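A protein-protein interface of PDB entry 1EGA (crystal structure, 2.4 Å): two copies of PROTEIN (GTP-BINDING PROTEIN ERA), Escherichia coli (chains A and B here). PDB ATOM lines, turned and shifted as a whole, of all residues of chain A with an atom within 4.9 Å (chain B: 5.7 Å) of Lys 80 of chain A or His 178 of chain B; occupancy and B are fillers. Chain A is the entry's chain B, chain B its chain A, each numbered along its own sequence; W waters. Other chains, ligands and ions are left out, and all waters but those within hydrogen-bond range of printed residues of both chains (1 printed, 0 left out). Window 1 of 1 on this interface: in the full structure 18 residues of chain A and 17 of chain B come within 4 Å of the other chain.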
ATOM      1  N   ASN A  75      -2.246  12.436   5.317  1.00  0.00           N
ATOM      2  CA  ASN A  75      -3.700  12.570   5.456  1.00  0.00           C
ATOM      3  C   ASN A  75      -4.132  12.329   6.906  1.00  0.00           C
ATOM      4  O   ASN A  75      -4.877  13.126   7.460  1.00  0.00           O
ATOM      5  CB  ASN A  75      -4.431  11.618   4.493  1.00  0.00           C
ATOM      6  CG  ASN A  75      -4.627  12.219   3.090  1.00  0.00           C
ATOM      7  OD1 ASN A  75      -4.739  13.449   2.912  1.00  0.00           O
ATOM      8  ND2 ASN A  75      -4.702  11.343   2.090  1.00  0.00           N
ATOM      9  N   ARG A  76      -3.632  11.252   7.515  1.00  0.00           N
ATOM     10  CA  ARG A  76      -3.918  10.922   8.926  1.00  0.00           C
ATOM     11  C   ARG A  76      -3.494  12.056   9.853  1.00  0.00           C
ATOM     12  O   ARG A  76      -4.163  12.358  10.841  1.00  0.00           O
ATOM     13  CB  ARG A  76      -3.157   9.669   9.351  1.00  0.00           C
ATOM     14  CG  ARG A  76      -3.708   8.360   8.800  1.00  0.00           C
ATOM     15  CD  ARG A  76      -2.650   7.246   8.784  1.00  0.00           C
ATOM     16  NE  ARG A  76      -1.634   7.412   9.825  1.00  0.00           N
ATOM     17  CZ  ARG A  76      -0.462   6.779   9.846  1.00  0.00           C
ATOM     18  NH1 ARG A  76      -0.149   5.919   8.882  1.00  0.00           N
ATOM     19  NH2 ARG A  76       0.409   7.033  10.817  1.00  0.00           N
ATOM     20  N   MET A  78      -3.500  15.066   9.108  1.00  0.00           N
ATOM     21  CA  MET A  78      -4.507  16.111   8.894  1.00  0.00           C
ATOM     22  C   MET A  78      -5.893  15.650   9.276  1.00  0.00           C
ATOM     23  O   MET A  78      -6.816  16.461   9.374  1.00  0.00           O
ATOM     24  CB  MET A  78      -4.553  16.527   7.425  1.00  0.00           C
ATOM     25  CG  MET A  78      -3.538  17.553   7.062  1.00  0.00           C
ATOM     26  SD  MET A  78      -3.695  18.088   5.364  1.00  0.00           S
ATOM     27  CE  MET A  78      -3.368  16.527   4.542  1.00  0.00           C
ATOM     28  N   ASN A  79      -6.024  14.344   9.489  1.00  0.00           N
ATOM     29  CA  ASN A  79      -7.298  13.723   9.827  1.00  0.00           C
ATOM     30  C   ASN A  79      -8.217  13.790   8.619  1.00  0.00           C
ATOM     31  O   ASN A  79      -9.381  14.178   8.713  1.00  0.00           O
ATOM     32  CB  ASN A  79      -7.951  14.429  11.017  1.00  0.00           C
ATOM     33  CG  ASN A  79      -7.121  14.337  12.265  1.00  0.00           C
ATOM     34  OD1 ASN A  79      -6.728  13.245  12.674  1.00  0.00           O
ATOM     35  ND2 ASN A  79      -6.831  15.482  12.876  1.00  0.00           N
ATOM     36  N   LYS A  80      -7.658  13.443   7.470  1.00  0.00           N
ATOM     37  CA  LYS A  80      -8.397  13.469   6.238  1.00  0.00           C
ATOM     38  C   LYS A  80      -8.538  12.072   5.691  1.00  0.00           C
ATOM     39  O   LYS A  80      -7.857  11.150   6.143  1.00  0.00           O
ATOM     40  CB  LYS A  80      -7.708  14.384   5.217  1.00  0.00           C
ATOM     41  CG  LYS A  80      -7.779  15.868   5.570  1.00  0.00           C
ATOM     42  CD  LYS A  80      -7.713  16.730   4.330  1.00  0.00           C
ATOM     43  CE  LYS A  80      -7.073  18.079   4.607  1.00  0.00           C
ATOM     44  NZ  LYS A  80      -8.017  19.235   4.644  1.00  0.00           N
ATOM     45  N   ALA A  81      -9.469  11.915   4.757  1.00  0.00           N
ATOM     46  CA  ALA A  81      -9.700  10.631   4.139  1.00  0.00           C
ATOM     47  C   ALA A  81      -8.456  10.196   3.370  1.00  0.00           C
ATOM     48  O   ALA A  81      -7.880  10.974   2.617  1.00  0.00           O
ATOM     49  CB  ALA A  81     -10.905  10.714   3.220  1.00  0.00           C
ATOM     50  N   ALA A  82      -8.043   8.951   3.581  1.00  0.00           N
ATOM     51  CA  ALA A  82      -6.865   8.383   2.936  1.00  0.00           C
ATOM     52  C   ALA A  82      -6.836   8.671   1.452  1.00  0.00           C
ATOM     53  O   ALA A  82      -5.766   8.779   0.862  1.00  0.00           O
ATOM     54  CB  ALA A  82      -6.832   6.891   3.161  1.00  0.00           C
ATOM     55  N   SER A  84      -8.051  11.433  -0.011  1.00  0.00           N
ATOM     56  CA  SER A  84      -7.804  12.842  -0.307  1.00  0.00           C
ATOM     57  C   SER A  84      -6.437  13.043  -0.974  1.00  0.00           C
ATOM     58  O   SER A  84      -5.407  12.621  -0.445  1.00  0.00           O
ATOM     59  CB  SER A  84      -7.899  13.680   0.956  1.00  0.00           C
ATOM     60  OG  SER A  84      -7.805  15.051   0.610  1.00  0.00           O
ATOM     61  N   HIS A 179      -3.214  22.708   2.102  1.00  0.00           N
ATOM     62  CA  HIS A 179      -3.628  21.447   2.704  1.00  0.00           C
ATOM     63  C   HIS A 179      -3.750  21.585   4.232  1.00  0.00           C
ATOM     64  O   HIS A 179      -4.545  20.883   4.863  1.00  0.00           O
ATOM     65  CB  HIS A 179      -2.566  20.362   2.496  1.00  0.00           C
ATOM     66  CG  HIS A 179      -2.489  19.792   1.116  1.00  0.00           C
ATOM     67  ND1 HIS A 179      -3.119  18.624   0.766  1.00  0.00           N
ATOM     68  CD2 HIS A 179      -1.701  20.126   0.058  1.00  0.00           C
ATOM     69  CE1 HIS A 179      -2.716  18.244  -0.438  1.00  0.00           C
ATOM     70  NE2 HIS A 179      -1.856  19.144  -0.879  1.00  0.00           N
ATOM     71  N   SER B   6      -9.198  12.345  -5.955  1.00  0.00           N
ATOM     72  CA  SER B   6     -10.209  12.644  -4.949  1.00  0.00           C
ATOM     73  C   SER B   6     -11.047  13.806  -5.462  1.00  0.00           C
ATOM     74  O   SER B   6     -10.598  14.545  -6.343  1.00  0.00           O
ATOM     75  CB  SER B   6      -9.564  13.001  -3.598  1.00  0.00           C
ATOM     76  OG  SER B   6      -8.995  14.303  -3.597  1.00  0.00           O
ATOM     77  N   TYR B   7     -12.262  13.957  -4.944  1.00  0.00           N
ATOM     78  CA  TYR B   7     -13.149  15.032  -5.385  1.00  0.00           C
ATOM     79  C   TYR B   7     -13.748  15.733  -4.210  1.00  0.00           C
ATOM     80  O   TYR B   7     -14.101  15.099  -3.214  1.00  0.00           O
ATOM     81  CB  TYR B   7     -14.287  14.486  -6.230  1.00  0.00           C
ATOM     82  CG  TYR B   7     -13.819  13.529  -7.287  1.00  0.00           C
ATOM     83  CD1 TYR B   7     -13.499  12.222  -6.952  1.00  0.00           C
ATOM     84  CD2 TYR B   7     -13.664  13.935  -8.615  1.00  0.00           C
ATOM     85  CE1 TYR B   7     -13.036  11.351  -7.886  1.00  0.00           C
ATOM     86  CE2 TYR B   7     -13.197  13.057  -9.571  1.00  0.00           C
ATOM     87  CZ  TYR B   7     -12.887  11.765  -9.193  1.00  0.00           C
ATOM     88  OH  TYR B   7     -12.442  10.852 -10.109  1.00  0.00           O
ATOM     89  N   CYS B   8     -13.903  17.040  -4.341  1.00  0.00           N
ATOM     90  CA  CYS B   8     -14.464  17.821  -3.263  1.00  0.00           C
ATOM     91  C   CYS B   8     -15.038  19.119  -3.805  1.00  0.00           C
ATOM     92  O   CYS B   8     -14.441  19.745  -4.677  1.00  0.00           O
ATOM     93  CB  CYS B   8     -13.372  18.073  -2.191  1.00  0.00           C
ATOM     94  SG  CYS B   8     -13.669  19.449  -1.061  1.00  0.00           S
ATOM     95  N   THR B  52     -18.454  13.309   3.825  1.00  0.00           N
ATOM     96  CA  THR B  52     -17.220  12.728   3.340  1.00  0.00           C
ATOM     97  C   THR B  52     -17.365  11.223   3.303  1.00  0.00           C
ATOM     98  O   THR B  52     -17.821  10.617   4.259  1.00  0.00           O
ATOM     99  CB  THR B  52     -16.034  13.083   4.273  1.00  0.00           C
ATOM    100  OG1 THR B  52     -15.933  14.509   4.419  1.00  0.00           O
ATOM    101  CG2 THR B  52     -14.738  12.513   3.717  1.00  0.00           C
ATOM    102  N   GLY B  54     -15.119   7.964   1.307  1.00  0.00           N
ATOM    103  CA  GLY B  54     -14.119   7.575   0.333  1.00  0.00           C
ATOM    104  C   GLY B  54     -13.401   8.806  -0.195  1.00  0.00           C
ATOM    105  O   GLY B  54     -13.028   9.694   0.582  1.00  0.00           O
ATOM    106  N   ALA B  55     -13.290   8.889  -1.521  1.00  0.00           N
ATOM    107  CA  ALA B  55     -12.626   9.994  -2.208  1.00  0.00           C
ATOM    108  C   ALA B  55     -13.512  11.221  -2.338  1.00  0.00           C
ATOM    109  O   ALA B  55     -13.052  12.269  -2.798  1.00  0.00           O
ATOM    110  CB  ALA B  55     -12.210   9.543  -3.592  1.00  0.00           C
ATOM    111  N   TYR B  56     -14.766  11.107  -1.905  1.00  0.00           N
ATOM    112  CA  TYR B  56     -15.722  12.199  -2.058  1.00  0.00           C
ATOM    113  C   TYR B  56     -16.037  12.968  -0.778  1.00  0.00           C
ATOM    114  O   TYR B  56     -16.280  12.379   0.265  1.00  0.00           O
ATOM    115  CB  TYR B  56     -17.017  11.637  -2.662  1.00  0.00           C
ATOM    116  CG  TYR B  56     -16.755  10.777  -3.870  1.00  0.00           C
ATOM    117  CD1 TYR B  56     -16.561  11.355  -5.131  1.00  0.00           C
ATOM    118  CD2 TYR B  56     -16.570   9.404  -3.734  1.00  0.00           C
ATOM    119  CE1 TYR B  56     -16.179  10.582  -6.229  1.00  0.00           C
ATOM    120  CE2 TYR B  56     -16.188   8.619  -4.819  1.00  0.00           C
ATOM    121  CZ  TYR B  56     -15.982   9.216  -6.059  1.00  0.00           C
ATOM    122  OH  TYR B  56     -15.526   8.463  -7.116  1.00  0.00           O
ATOM    123  N   GLN B  57     -16.058  14.297  -0.907  1.00  0.00           N
ATOM    124  CA  GLN B  57     -16.396  15.207   0.175  1.00  0.00           C
ATOM    125  C   GLN B  57     -17.269  16.342  -0.342  1.00  0.00           C
ATOM    126  O   GLN B  57     -16.798  17.280  -0.979  1.00  0.00           O
ATOM    127  CB  GLN B  57     -15.153  15.799   0.856  1.00  0.00           C
ATOM    128  CG  GLN B  57     -15.457  16.992   1.820  1.00  0.00           C
ATOM    129  CD  GLN B  57     -14.272  17.383   2.721  1.00  0.00           C
ATOM    130  OE1 GLN B  57     -13.924  18.559   2.823  1.00  0.00           O
ATOM    131  NE2 GLN B  57     -13.639  16.392   3.350  1.00  0.00           N
ATOM    132  N   LYS B  80      -7.426  28.383   8.413  1.00  0.00           N
ATOM    133  CA  LYS B  80      -6.556  28.515   7.261  1.00  0.00           C
ATOM    134  C   LYS B  80      -6.404  29.959   6.864  1.00  0.00           C
ATOM    135  O   LYS B  80      -7.253  30.804   7.173  1.00  0.00           O
ATOM    136  CB  LYS B  80      -7.108  27.730   6.074  1.00  0.00           C
ATOM    137  CG  LYS B  80      -7.098  26.220   6.277  1.00  0.00           C
ATOM    138  CD  LYS B  80      -6.787  25.510   4.970  1.00  0.00           C
ATOM    139  CE  LYS B  80      -7.519  24.187   4.828  1.00  0.00           C
ATOM    140  NZ  LYS B  80      -6.628  22.997   4.852  1.00  0.00           N
ATOM    141  N   ALA B 176     -10.431  17.341  -6.724  1.00  0.00           N
ATOM    142  CA  ALA B 176      -9.688  18.181  -5.797  1.00  0.00           C
ATOM    143  C   ALA B 176      -9.453  17.468  -4.470  1.00  0.00           C
ATOM    144  O   ALA B 176     -10.058  16.436  -4.162  1.00  0.00           O
ATOM    145  CB  ALA B 176     -10.452  19.498  -5.551  1.00  0.00           C
ATOM    146  N   THR B 177      -8.545  18.032  -3.690  1.00  0.00           N
ATOM    147  CA  THR B 177      -8.232  17.494  -2.384  1.00  0.00           C
ATOM    148  C   THR B 177      -9.320  17.961  -1.420  1.00  0.00           C
ATOM    149  O   THR B 177      -9.901  19.042  -1.608  1.00  0.00           O
ATOM    150  CB  THR B 177      -6.822  18.007  -1.920  1.00  0.00           C
ATOM    151  OG1 THR B 177      -6.322  17.206  -0.836  1.00  0.00           O
ATOM    152  CG2 THR B 177      -6.893  19.479  -1.502  1.00  0.00           C
ATOM    153  N   HIS B 178      -9.633  17.148  -0.420  1.00  0.00           N
ATOM    154  CA  HIS B 178     -10.646  17.552   0.537  1.00  0.00           C
ATOM    155  C   HIS B 178     -10.180  18.801   1.268  1.00  0.00           C
ATOM    156  O   HIS B 178      -9.007  18.928   1.560  1.00  0.00           O
ATOM    157  CB  HIS B 178     -10.897  16.444   1.571  1.00  0.00           C
ATOM    158  CG  HIS B 178     -11.393  15.159   0.985  1.00  0.00           C
ATOM    159  ND1 HIS B 178     -11.658  14.987  -0.354  1.00  0.00           N
ATOM    160  CD2 HIS B 178     -11.638  13.953   1.572  1.00  0.00           C
ATOM    161  CE1 HIS B 178     -12.034  13.740  -0.579  1.00  0.00           C
ATOM    162  NE2 HIS B 178     -12.028  13.093   0.580  1.00  0.00           N
ATOM    163  N   HIS B 179     -11.083  19.737   1.523  1.00  0.00           N
ATOM    164  CA  HIS B 179     -10.754  20.942   2.282  1.00  0.00           C
ATOM    165  C   HIS B 179     -10.785  20.670   3.799  1.00  0.00           C
ATOM    166  O   HIS B 179     -10.032  21.282   4.571  1.00  0.00           O
ATOM    167  CB  HIS B 179     -11.804  22.020   2.058  1.00  0.00           C
ATOM    168  CG  HIS B 179     -11.662  22.768   0.781  1.00  0.00           C
ATOM    169  ND1 HIS B 179     -11.014  23.995   0.713  1.00  0.00           N
ATOM    170  CD2 HIS B 179     -12.170  22.547  -0.442  1.00  0.00           C
ATOM    171  CE1 HIS B 179     -11.151  24.481  -0.497  1.00  0.00           C
ATOM    172  NE2 HIS B 179     -11.847  23.633  -1.230  1.00  0.00           N
ATOM    173  N   PHE B 180     -11.675  19.769   4.214  1.00  0.00           N
ATOM    174  CA  PHE B 180     -11.892  19.484   5.629  1.00  0.00           C
ATOM    175  C   PHE B 180     -11.459  18.097   6.097  1.00  0.00           C
ATOM    176  O   PHE B 180     -11.401  17.137   5.308  1.00  0.00           O
ATOM    177  CB  PHE B 180     -13.396  19.616   5.968  1.00  0.00           C
ATOM    178  CG  PHE B 180     -13.935  21.021   5.882  1.00  0.00           C
ATOM    179  CD1 PHE B 180     -14.476  21.505   4.706  1.00  0.00           C
ATOM    180  CD2 PHE B 180     -13.928  21.848   6.996  1.00  0.00           C
ATOM    181  CE1 PHE B 180     -15.003  22.805   4.642  1.00  0.00           C
ATOM    182  CE2 PHE B 180     -14.451  23.149   6.945  1.00  0.00           C
ATOM    183  CZ  PHE B 180     -14.992  23.625   5.765  1.00  0.00           C
ATOM    184  N   PRO B 181     -11.076  17.995   7.394  1.00  0.00           N
ATOM    185  CA  PRO B 181     -10.684  16.704   7.950  1.00  0.00           C
ATOM    186  C   PRO B 181     -12.053  15.995   7.983  1.00  0.00           C
ATOM    187  O   PRO B 181     -13.098  16.656   7.946  1.00  0.00           O
ATOM    188  CB  PRO B 181     -10.211  17.062   9.353  1.00  0.00           C
ATOM    189  CG  PRO B 181      -9.773  18.468   9.206  1.00  0.00           C
ATOM    190  CD  PRO B 181     -10.838  19.063   8.384  1.00  0.00           C
ATOM    191  N   GLU B 182     -12.049  14.676   8.095  1.00  0.00           N
ATOM    192  CA  GLU B 182     -13.262  13.901   8.077  1.00  0.00           C
ATOM    193  C   GLU B 182     -14.387  14.393   8.968  1.00  0.00           C
ATOM    194  O   GLU B 182     -15.380  14.915   8.459  1.00  0.00           O
ATOM    195  CB  GLU B 182     -12.954  12.449   8.381  1.00  0.00           C
ATOM    196  CG  GLU B 182     -12.294  11.770   7.230  1.00  0.00           C
ATOM    197  CD  GLU B 182     -12.381  10.267   7.322  1.00  0.00           C
ATOM    198  OE1 GLU B 182     -11.653   9.664   8.147  1.00  0.00           O
ATOM    199  OE2 GLU B 182     -13.188   9.690   6.552  1.00  0.00           O
HETATM  200  O   HOH W   1      -5.318  15.860   1.640  1.00  0.00           O
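Water W1 lies within hydrogen-bond range of the side-chain amide oxygen (OD1) of Asn 75 of chain A (2.8 Å), the side-chain hydroxyl (OG) of Ser 84 of chain A (2.8 Å) and the side-chain hydroxyl (OG1) of Thr 177 of chain B (3.0 Å).
The side-chain amino group (NZ) of Lys 80 of chain A sits at hydrogen-bond distance from the backbone carbonyl oxygen (O) of His 179 of chain B (2.9 Å). O of Asn 79 of chain A sits at hydrogen-bond distance from N of Glu 182 of chain B, 2.8 Å away. The side-chain amino group (NZ) of Lys 80 of chain B sits at hydrogen-bond distance from the backbone carbonyl oxygen (O) of His 179 of chain A (3.0 Å). The side-chain hydroxyl of Ser 84 of chain A lies within hydrogen-bond range of the backbone NH of His 178 of chain B (3.0 Å). The backbone carbonyl oxygen (O) of His 178 of chain B lies within hydrogen-bond range of the side-chain amino group (NZ) of Lys 80 of chain A (3.3 Å). OG1 of Thr 177 of chain B is in hydrogen-bond range of OG of Ser 84 of chain A (3.0 Å).
The backbone NH (N) of Phe 180 of chain B is in hydrogen-bond range of the side-chain amide oxygen (OE1) of Gln 57 of chain B (2.9 Å). ND2 of Asn 75 of chain A lies within hydrogen-bond range of O of Ala 81 of chain A, at 3.2 Å. O of Arg 76 of chain A lies close to OD1 of Asn 79 of chain A (3.3 Å). N of Lys 80 of chain A sits at hydrogen-bond distance from O of Asn 75 of chain A (2.8 Å). The side-chain amide oxygen (OE1) of Gln 57 of chain B lies within hydrogen-bond range of the backbone NH (N) of His 179 of chain B, at 3.3 Å. The backbone carbonyl oxygen of Ser 84 of chain A lies within hydrogen-bond range of the side-chain amide nitrogen of Asn 75 of chain A, 2.9 Å away.
Lys 80 of chain A touches His 179 of chain B, and with the chains exchanged His 179 of chain A touches Lys 80 of chain B. Of the 15 pairs that touch across the chains among the printed residues, 2 have their exchanged pair printed and touching as well.
Along chain B the printed residues that touch a printed residue of chain A span positions 6 to 182. Of the 9 printed residues of chain A, 6 touch a printed residue of chain B. Printed residues of chain A that touch a printed residue of chain B: Met 78, Asn 79, Lys 80, Ala 81, Ser 84 and His 179. Among the printed residues, 15 pairs touch across the chains. Among the printed residues, no Asp or Glu carboxylate lies within 4 Å of a Lys or Arg side-chain nitrogen of the other chain.
O of Met 78 of chain A touches CB of Pro 181 of chain B, 3.4 Å away. Asn 79 of chain A touches Pro 181 of chain B. N of Phe 180 of chain B touches NZ of Lys 80 of chain A (3.7 Å). CG of Lys 80 of chain A touches CA of Pro 181 of chain B, at 3.8 Å. Gly 54 of chain B touches Ala 81 of chain A (O to CB, 3.5 Å). Ala 81 of chain A touches His 178 of chain B. N of Ala 81 of chain A touches CG of Glu 182 of chain B, at 3.8 Å. Ser 84 of chain A touches Ser 6 of chain B (CA to CB, 3.7 Å). OG1 of Thr 177 of chain B touches CE1 of His 179 of chain A, at 3.8 Å.
Printed residues of chain B within 4 Å of Met 78 of chain A: Pro 181 (3.4 Å). Of the printed residues of chain B, Ser 84 of chain A touches Ser 6, Thr 177 and His 178. Of the printed residues of chain B, His 179 of chain A touches Lys 80 and Thr 177. Of the printed residues of chain A, Ser 6 of chain B touches Ser 84. Of chain A, only Lys 80, Ala 81 and Ser 84 come within 4 Å of His 178 of chain B. The nearest printed residue of chain B that does not touch Ser 84 of chain A is Ala 55 of chain B (5.3 Å).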
